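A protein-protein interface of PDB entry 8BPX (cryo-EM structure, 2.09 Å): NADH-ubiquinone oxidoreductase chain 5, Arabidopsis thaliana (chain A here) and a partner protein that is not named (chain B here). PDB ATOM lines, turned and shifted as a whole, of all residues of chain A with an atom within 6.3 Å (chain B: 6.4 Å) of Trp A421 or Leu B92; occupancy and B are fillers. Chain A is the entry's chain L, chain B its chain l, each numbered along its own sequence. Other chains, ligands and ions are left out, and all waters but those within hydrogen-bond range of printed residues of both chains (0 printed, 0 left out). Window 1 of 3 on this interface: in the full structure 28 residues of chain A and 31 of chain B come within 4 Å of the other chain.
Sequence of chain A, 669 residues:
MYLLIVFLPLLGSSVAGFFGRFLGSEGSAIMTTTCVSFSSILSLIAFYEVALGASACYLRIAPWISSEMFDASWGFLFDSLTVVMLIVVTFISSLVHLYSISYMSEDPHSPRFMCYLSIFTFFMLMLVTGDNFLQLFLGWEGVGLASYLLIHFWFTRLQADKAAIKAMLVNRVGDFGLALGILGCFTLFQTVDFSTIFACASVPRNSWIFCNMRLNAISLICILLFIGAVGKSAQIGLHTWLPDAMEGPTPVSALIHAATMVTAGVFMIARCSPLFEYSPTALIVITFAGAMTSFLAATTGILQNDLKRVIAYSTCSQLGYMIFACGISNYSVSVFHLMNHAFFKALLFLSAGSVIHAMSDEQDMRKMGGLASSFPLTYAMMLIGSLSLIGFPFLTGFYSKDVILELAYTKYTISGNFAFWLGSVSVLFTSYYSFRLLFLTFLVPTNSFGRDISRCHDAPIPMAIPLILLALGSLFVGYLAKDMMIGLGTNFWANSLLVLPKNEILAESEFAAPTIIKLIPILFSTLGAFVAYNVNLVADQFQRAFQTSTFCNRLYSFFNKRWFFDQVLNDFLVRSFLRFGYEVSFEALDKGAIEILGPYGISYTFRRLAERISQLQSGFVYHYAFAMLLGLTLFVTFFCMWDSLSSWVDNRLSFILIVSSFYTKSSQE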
ATOM      1  N   GLY A 416     -33.310 -27.166   2.236  1.00  0.00           N
ATOM      2  CA  GLY A 416     -32.987 -25.750   2.285  1.00  0.00           C
ATOM      3  C   GLY A 416     -31.605 -25.493   2.855  1.00  0.00           C
ATOM      4  O   GLY A 416     -30.836 -24.694   2.318  1.00  0.00           O
ATOM      5  N   ASN A 417     -31.273 -26.175   3.950  1.00  0.00           N
ATOM      6  CA  ASN A 417     -29.940 -26.071   4.536  1.00  0.00           C
ATOM      7  C   ASN A 417     -28.865 -26.551   3.567  1.00  0.00           C
ATOM      8  O   ASN A 417     -27.815 -25.906   3.411  1.00  0.00           O
ATOM      9  CB  ASN A 417     -29.902 -26.877   5.832  1.00  0.00           C
ATOM     10  CG  ASN A 417     -28.780 -26.463   6.745  1.00  0.00           C
ATOM     11  OD1 ASN A 417     -28.341 -27.241   7.584  1.00  0.00           O
ATOM     12  ND2 ASN A 417     -28.289 -25.245   6.571  1.00  0.00           N
ATOM     13  N   PHE A 418     -29.119 -27.681   2.911  1.00  0.00           N
ATOM     14  CA  PHE A 418     -28.194 -28.222   1.922  1.00  0.00           C
ATOM     15  C   PHE A 418     -27.916 -27.199   0.825  1.00  0.00           C
ATOM     16  O   PHE A 418     -26.754 -26.923   0.485  1.00  0.00           O
ATOM     17  CB  PHE A 418     -28.801 -29.509   1.357  1.00  0.00           C
ATOM     18  CG  PHE A 418     -27.905 -30.277   0.436  1.00  0.00           C
ATOM     19  CD1 PHE A 418     -26.953 -31.145   0.944  1.00  0.00           C
ATOM     20  CD2 PHE A 418     -28.037 -30.159  -0.934  1.00  0.00           C
ATOM     21  CE1 PHE A 418     -26.141 -31.874   0.099  1.00  0.00           C
ATOM     22  CE2 PHE A 418     -27.228 -30.888  -1.785  1.00  0.00           C
ATOM     23  CZ  PHE A 418     -26.274 -31.743  -1.265  1.00  0.00           C
ATOM     24  N   ALA A 419     -28.922 -26.534   0.303  1.00  0.00           N
ATOM     25  CA  ALA A 419     -28.842 -25.559  -0.780  1.00  0.00           C
ATOM     26  C   ALA A 419     -28.152 -24.285  -0.320  1.00  0.00           C
ATOM     27  O   ALA A 419     -27.325 -23.767  -1.044  1.00  0.00           O
ATOM     28  CB  ALA A 419     -30.187 -25.294  -1.362  1.00  0.00           C
ATOM     29  N   PHE A 420     -28.425 -23.908   0.902  1.00  0.00           N
ATOM     30  CA  PHE A 420     -27.746 -22.723   1.413  1.00  0.00           C
ATOM     31  C   PHE A 420     -26.242 -22.950   1.489  1.00  0.00           C
ATOM     32  O   PHE A 420     -25.455 -22.139   0.987  1.00  0.00           O
ATOM     33  CB  PHE A 420     -28.302 -22.336   2.780  1.00  0.00           C
ATOM     34  CG  PHE A 420     -27.567 -21.201   3.422  1.00  0.00           C
ATOM     35  CD1 PHE A 420     -27.577 -19.945   2.847  1.00  0.00           C
ATOM     36  CD2 PHE A 420     -26.841 -21.393   4.583  1.00  0.00           C
ATOM     37  CE1 PHE A 420     -26.900 -18.897   3.430  1.00  0.00           C
ATOM     38  CE2 PHE A 420     -26.161 -20.345   5.171  1.00  0.00           C
ATOM     39  CZ  PHE A 420     -26.189 -19.099   4.590  1.00  0.00           C
ATOM     40  N   TRP A 421     -25.828 -24.075   2.081  1.00  0.00           N
ATOM     41  CA  TRP A 421     -24.400 -24.379   2.171  1.00  0.00           C
ATOM     42  C   TRP A 421     -23.752 -24.437   0.789  1.00  0.00           C
ATOM     43  O   TRP A 421     -22.717 -23.793   0.540  1.00  0.00           O
ATOM     44  CB  TRP A 421     -24.187 -25.707   2.899  1.00  0.00           C
ATOM     45  CG  TRP A 421     -24.432 -25.671   4.373  1.00  0.00           C
ATOM     46  CD1 TRP A 421     -24.421 -24.574   5.184  1.00  0.00           C
ATOM     47  CD2 TRP A 421     -24.698 -26.792   5.219  1.00  0.00           C
ATOM     48  NE1 TRP A 421     -24.676 -24.942   6.479  1.00  0.00           N
ATOM     49  CE2 TRP A 421     -24.847 -26.300   6.530  1.00  0.00           C
ATOM     50  CE3 TRP A 421     -24.829 -28.167   4.995  1.00  0.00           C
ATOM     51  CZ2 TRP A 421     -25.123 -27.130   7.611  1.00  0.00           C
ATOM     52  CZ3 TRP A 421     -25.106 -28.990   6.070  1.00  0.00           C
ATOM     53  CH2 TRP A 421     -25.247 -28.470   7.361  1.00  0.00           C
ATOM     54  N   LEU A 422     -24.352 -25.207  -0.127  1.00  0.00           N
ATOM     55  CA  LEU A 422     -23.712 -25.428  -1.421  1.00  0.00           C
ATOM     56  C   LEU A 422     -23.642 -24.144  -2.242  1.00  0.00           C
ATOM     57  O   LEU A 422     -22.594 -23.836  -2.820  1.00  0.00           O
ATOM     58  CB  LEU A 422     -24.435 -26.536  -2.182  1.00  0.00           C
ATOM     59  CG  LEU A 422     -23.956 -27.947  -1.830  1.00  0.00           C
ATOM     60  CD1 LEU A 422     -24.492 -28.973  -2.814  1.00  0.00           C
ATOM     61  CD2 LEU A 422     -22.432 -28.011  -1.765  1.00  0.00           C
ATOM     62  N   GLY A 423     -24.732 -23.374  -2.295  1.00  0.00           N
ATOM     63  CA  GLY A 423     -24.697 -22.107  -3.003  1.00  0.00           C
ATOM     64  C   GLY A 423     -23.708 -21.122  -2.414  1.00  0.00           C
ATOM     65  O   GLY A 423     -23.008 -20.415  -3.155  1.00  0.00           O
ATOM     66  N   SER A 424     -23.609 -21.077  -1.081  1.00  0.00           N
ATOM     67  CA  SER A 424     -22.649 -20.183  -0.444  1.00  0.00           C
ATOM     68  C   SER A 424     -21.224 -20.509  -0.869  1.00  0.00           C
ATOM     69  O   SER A 424     -20.476 -19.618  -1.287  1.00  0.00           O
ATOM     70  CB  SER A 424     -22.798 -20.256   1.078  1.00  0.00           C
ATOM     71  OG  SER A 424     -24.151 -20.086   1.460  1.00  0.00           O
ATOM     72  N   VAL A 425     -20.828 -21.783  -0.796  1.00  0.00           N
ATOM     73  CA  VAL A 425     -19.452 -22.105  -1.188  1.00  0.00           C
ATOM     74  C   VAL A 425     -19.250 -21.921  -2.697  1.00  0.00           C
ATOM     75  O   VAL A 425     -18.157 -21.524  -3.161  1.00  0.00           O
ATOM     76  CB  VAL A 425     -19.073 -23.520  -0.703  1.00  0.00           C
ATOM     77  CG1 VAL A 425     -19.833 -24.596  -1.455  1.00  0.00           C
ATOM     78  CG2 VAL A 425     -17.570 -23.737  -0.805  1.00  0.00           C
ATOM     79  N   SER A 426     -20.297 -22.165  -3.488  1.00  0.00           N
ATOM     80  CA  SER A 426     -20.177 -21.992  -4.927  1.00  0.00           C
ATOM     81  C   SER A 426     -19.935 -20.537  -5.295  1.00  0.00           C
ATOM     82  O   SER A 426     -19.309 -20.263  -6.320  1.00  0.00           O
ATOM     83  CB  SER A 426     -21.426 -22.526  -5.626  1.00  0.00           C
ATOM     84  OG  SER A 426     -21.501 -23.933  -5.502  1.00  0.00           O
ATOM     85  N   GLY B  87     -20.143 -39.251  -2.590  1.00  0.00           N
ATOM     86  CA  GLY B  87     -20.214 -39.468  -1.159  1.00  0.00           C
ATOM     87  C   GLY B  87     -20.010 -38.194  -0.370  1.00  0.00           C
ATOM     88  O   GLY B  87     -20.487 -38.079   0.757  1.00  0.00           O
ATOM     89  N   PHE B  88     -19.296 -37.225  -0.946  1.00  0.00           N
ATOM     90  CA  PHE B  88     -19.289 -35.880  -0.374  1.00  0.00           C
ATOM     91  C   PHE B  88     -20.706 -35.321  -0.257  1.00  0.00           C
ATOM     92  O   PHE B  88     -21.094 -34.792   0.792  1.00  0.00           O
ATOM     93  CB  PHE B  88     -18.430 -34.944  -1.219  1.00  0.00           C
ATOM     94  CG  PHE B  88     -18.489 -33.512  -0.778  1.00  0.00           C
ATOM     95  CD1 PHE B  88     -18.132 -33.151   0.510  1.00  0.00           C
ATOM     96  CD2 PHE B  88     -18.967 -32.533  -1.635  1.00  0.00           C
ATOM     97  CE1 PHE B  88     -18.206 -31.832   0.917  1.00  0.00           C
ATOM     98  CE2 PHE B  88     -19.044 -31.215  -1.232  1.00  0.00           C
ATOM     99  CZ  PHE B  88     -18.663 -30.865   0.047  1.00  0.00           C
ATOM    100  N   PHE B  89     -21.492 -35.415  -1.335  1.00  0.00           N
ATOM    101  CA  PHE B  89     -22.863 -34.917  -1.297  1.00  0.00           C
ATOM    102  C   PHE B  89     -23.703 -35.696  -0.293  1.00  0.00           C
ATOM    103  O   PHE B  89     -24.530 -35.117   0.421  1.00  0.00           O
ATOM    104  CB  PHE B  89     -23.499 -34.994  -2.686  1.00  0.00           C
ATOM    105  CG  PHE B  89     -22.946 -34.004  -3.665  1.00  0.00           C
ATOM    106  CD1 PHE B  89     -22.713 -32.695  -3.291  1.00  0.00           C
ATOM    107  CD2 PHE B  89     -22.668 -34.385  -4.967  1.00  0.00           C
ATOM    108  CE1 PHE B  89     -22.208 -31.786  -4.189  1.00  0.00           C
ATOM    109  CE2 PHE B  89     -22.162 -33.478  -5.871  1.00  0.00           C
ATOM    110  CZ  PHE B  89     -21.931 -32.174  -5.481  1.00  0.00           C
ATOM    111  N   VAL B  90     -23.508 -37.014  -0.235  1.00  0.00           N
ATOM    112  CA  VAL B  90     -24.233 -37.828   0.741  1.00  0.00           C
ATOM    113  C   VAL B  90     -23.890 -37.393   2.164  1.00  0.00           C
ATOM    114  O   VAL B  90     -24.775 -37.257   3.019  1.00  0.00           O
ATOM    115  CB  VAL B  90     -23.942 -39.324   0.518  1.00  0.00           C
ATOM    116  CG1 VAL B  90     -24.233 -40.125   1.782  1.00  0.00           C
ATOM    117  CG2 VAL B  90     -24.750 -39.854  -0.649  1.00  0.00           C
ATOM    118  N   GLY B  91     -22.604 -37.169   2.438  1.00  0.00           N
ATOM    119  CA  GLY B  91     -22.194 -36.734   3.763  1.00  0.00           C
ATOM    120  C   GLY B  91     -22.729 -35.363   4.122  1.00  0.00           C
ATOM    121  O   GLY B  91     -23.101 -35.113   5.268  1.00  0.00           O
ATOM    122  N   LEU B  92     -22.789 -34.459   3.141  1.00  0.00           N
ATOM    123  CA  LEU B  92     -23.387 -33.148   3.380  1.00  0.00           C
ATOM    124  C   LEU B  92     -24.878 -33.266   3.684  1.00  0.00           C
ATOM    125  O   LEU B  92     -25.401 -32.557   4.551  1.00  0.00           O
ATOM    126  CB  LEU B  92     -23.155 -32.240   2.178  1.00  0.00           C
ATOM    127  CG  LEU B  92     -23.148 -30.745   2.482  1.00  0.00           C
ATOM    128  CD1 LEU B  92     -21.840 -30.350   3.142  1.00  0.00           C
ATOM    129  CD2 LEU B  92     -23.387 -29.938   1.221  1.00  0.00           C
ATOM    130  N   GLY B  93     -25.577 -34.155   2.977  1.00  0.00           N
ATOM    131  CA  GLY B  93     -26.983 -34.380   3.275  1.00  0.00           C
ATOM    132  C   GLY B  93     -27.207 -34.938   4.668  1.00  0.00           C
ATOM    133  O   GLY B  93     -28.117 -34.509   5.382  1.00  0.00           O
ATOM    134  N   LEU B  94     -26.379 -35.904   5.073  1.00  0.00           N
ATOM    135  CA  LEU B  94     -26.498 -36.453   6.421  1.00  0.00           C
ATOM    136  C   LEU B  94     -26.163 -35.399   7.470  1.00  0.00           C
ATOM    137  O   LEU B  94     -26.779 -35.362   8.540  1.00  0.00           O
ATOM    138  CB  LEU B  94     -25.597 -37.676   6.587  1.00  0.00           C
ATOM    139  CG  LEU B  94     -25.799 -38.824   5.595  1.00  0.00           C
ATOM    140  CD1 LEU B  94     -24.622 -39.782   5.642  1.00  0.00           C
ATOM    141  CD2 LEU B  94     -27.102 -39.551   5.865  1.00  0.00           C
ATOM    142  N   LEU B  95     -25.184 -34.544   7.180  1.00  0.00           N
ATOM    143  CA  LEU B  95     -24.867 -33.447   8.084  1.00  0.00           C
ATOM    144  C   LEU B  95     -26.040 -32.486   8.214  1.00  0.00           C
ATOM    145  O   LEU B  95     -26.318 -31.987   9.306  1.00  0.00           O
ATOM    146  CB  LEU B  95     -23.620 -32.718   7.596  1.00  0.00           C
ATOM    147  CG  LEU B  95     -22.334 -33.201   8.249  1.00  0.00           C
ATOM    148  CD1 LEU B  95     -21.130 -32.811   7.409  1.00  0.00           C
ATOM    149  CD2 LEU B  95     -22.227 -32.640   9.650  1.00  0.00           C
ATOM    150  N   ALA B  96     -26.730 -32.206   7.108  1.00  0.00           N
ATOM    151  CA  ALA B  96     -27.908 -31.348   7.181  1.00  0.00           C
ATOM    152  C   ALA B  96     -29.027 -32.012   7.974  1.00  0.00           C
ATOM    153  O   ALA B  96     -29.784 -31.332   8.673  1.00  0.00           O
ATOM    154  CB  ALA B  96     -28.384 -30.978   5.778  1.00  0.00           C
ATOM    155  N   VAL B  97     -29.162 -33.336   7.860  1.00  0.00           N
ATOM    156  CA  VAL B  97     -30.115 -34.060   8.702  1.00  0.00           C
ATOM    157  C   VAL B  97     -29.751 -33.891  10.173  1.00  0.00           C
ATOM    158  O   VAL B  97     -30.604 -33.577  11.013  1.00  0.00           O
ATOM    159  CB  VAL B  97     -30.165 -35.550   8.314  1.00  0.00           C
ATOM    160  CG1 VAL B  97     -30.813 -36.356   9.429  1.00  0.00           C
ATOM    161  CG2 VAL B  97     -30.895 -35.754   6.997  1.00  0.00           C
ATOM    162  N   ASN B  99     -28.088 -31.567  11.529  1.00  0.00           N
ATOM    163  CA  ASN B  99     -28.209 -30.175  11.945  1.00  0.00           C
ATOM    164  C   ASN B  99     -29.607 -29.874  12.469  1.00  0.00           C
ATOM    165  O   ASN B  99     -29.765 -29.099  13.417  1.00  0.00           O
ATOM    166  CB  ASN B  99     -27.859 -29.256  10.776  1.00  0.00           C
ATOM    167  CG  ASN B  99     -27.505 -27.853  11.221  1.00  0.00           C
ATOM    168  OD1 ASN B  99     -26.896 -27.663  12.268  1.00  0.00           O
ATOM    169  ND2 ASN B  99     -27.882 -26.866  10.422  1.00  0.00           N
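The side-chain amide nitrogen (ND2) of Asn B99 sits at hydrogen-bond distance from the side-chain amide oxygen (OD1) of Asn A417 (2.9 Å).
The side-chain hydroxyl (OG) of Ser A426 sits at hydrogen-bond distance from the backbone carbonyl oxygen (O) of Leu A422 (2.9 Å).
Among the printed residues, merely in contact across the chains: Phe A418 with Leu B92 (3.5 Å), Phe A418 with Phe B89 (3.6 Å), Leu A422 with Leu B92 (3.7 Å), Phe A418 with Gly B93 (3.7 Å), Trp A421 with Ala B96 (3.7 Å), Leu A422 with Phe B89 (3.9 Å), Trp A421 with Leu B92 (3.9 Å) and Trp A421 with Asn B99 (3.9 Å).
Of chain B, only Leu B92 (3.9 Å), Ala B96 (3.7 Å) and Asn B99 (3.9 Å) come within 4 Å of Trp A421. Of the printed residues of chain A, Leu B92 touches Phe A418 (3.5 Å), Trp A421 (3.9 Å) and Leu A422 (3.7 Å). Of the printed residues of chain B, Phe A418 touches Phe B89, Leu B92 and Gly B93. Of the printed residues of chain A, Gly B93 touches Phe A418. Of the printed residues of chain A, Ala B96 touches Trp A421 (3.7 Å). Leu B95 touches none of the printed residues of chain A. Phe A420 touches none of the printed residues of chain B. The nearest residue of chain B that does not touch Trp A421 is Leu B95 (4.2 Å). The nearest printed residue of chain A that does not touch Leu B92 is Asn A417 (6.4 Å). The nearest printed residue of chain A that does not touch Asn B99 is Phe A418 (7.7 Å).
Hydrophobic or aromatic side chains of chain A within 4 Å of the printed part of chain B: Phe A418, Trp A421 and Leu A422. Among the printed residues, 9 pairs touch across the chains. Among the printed residues, no Asp or Glu carboxylate lies within 4 Å of a Lys or Arg side-chain nitrogen of the other chain.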
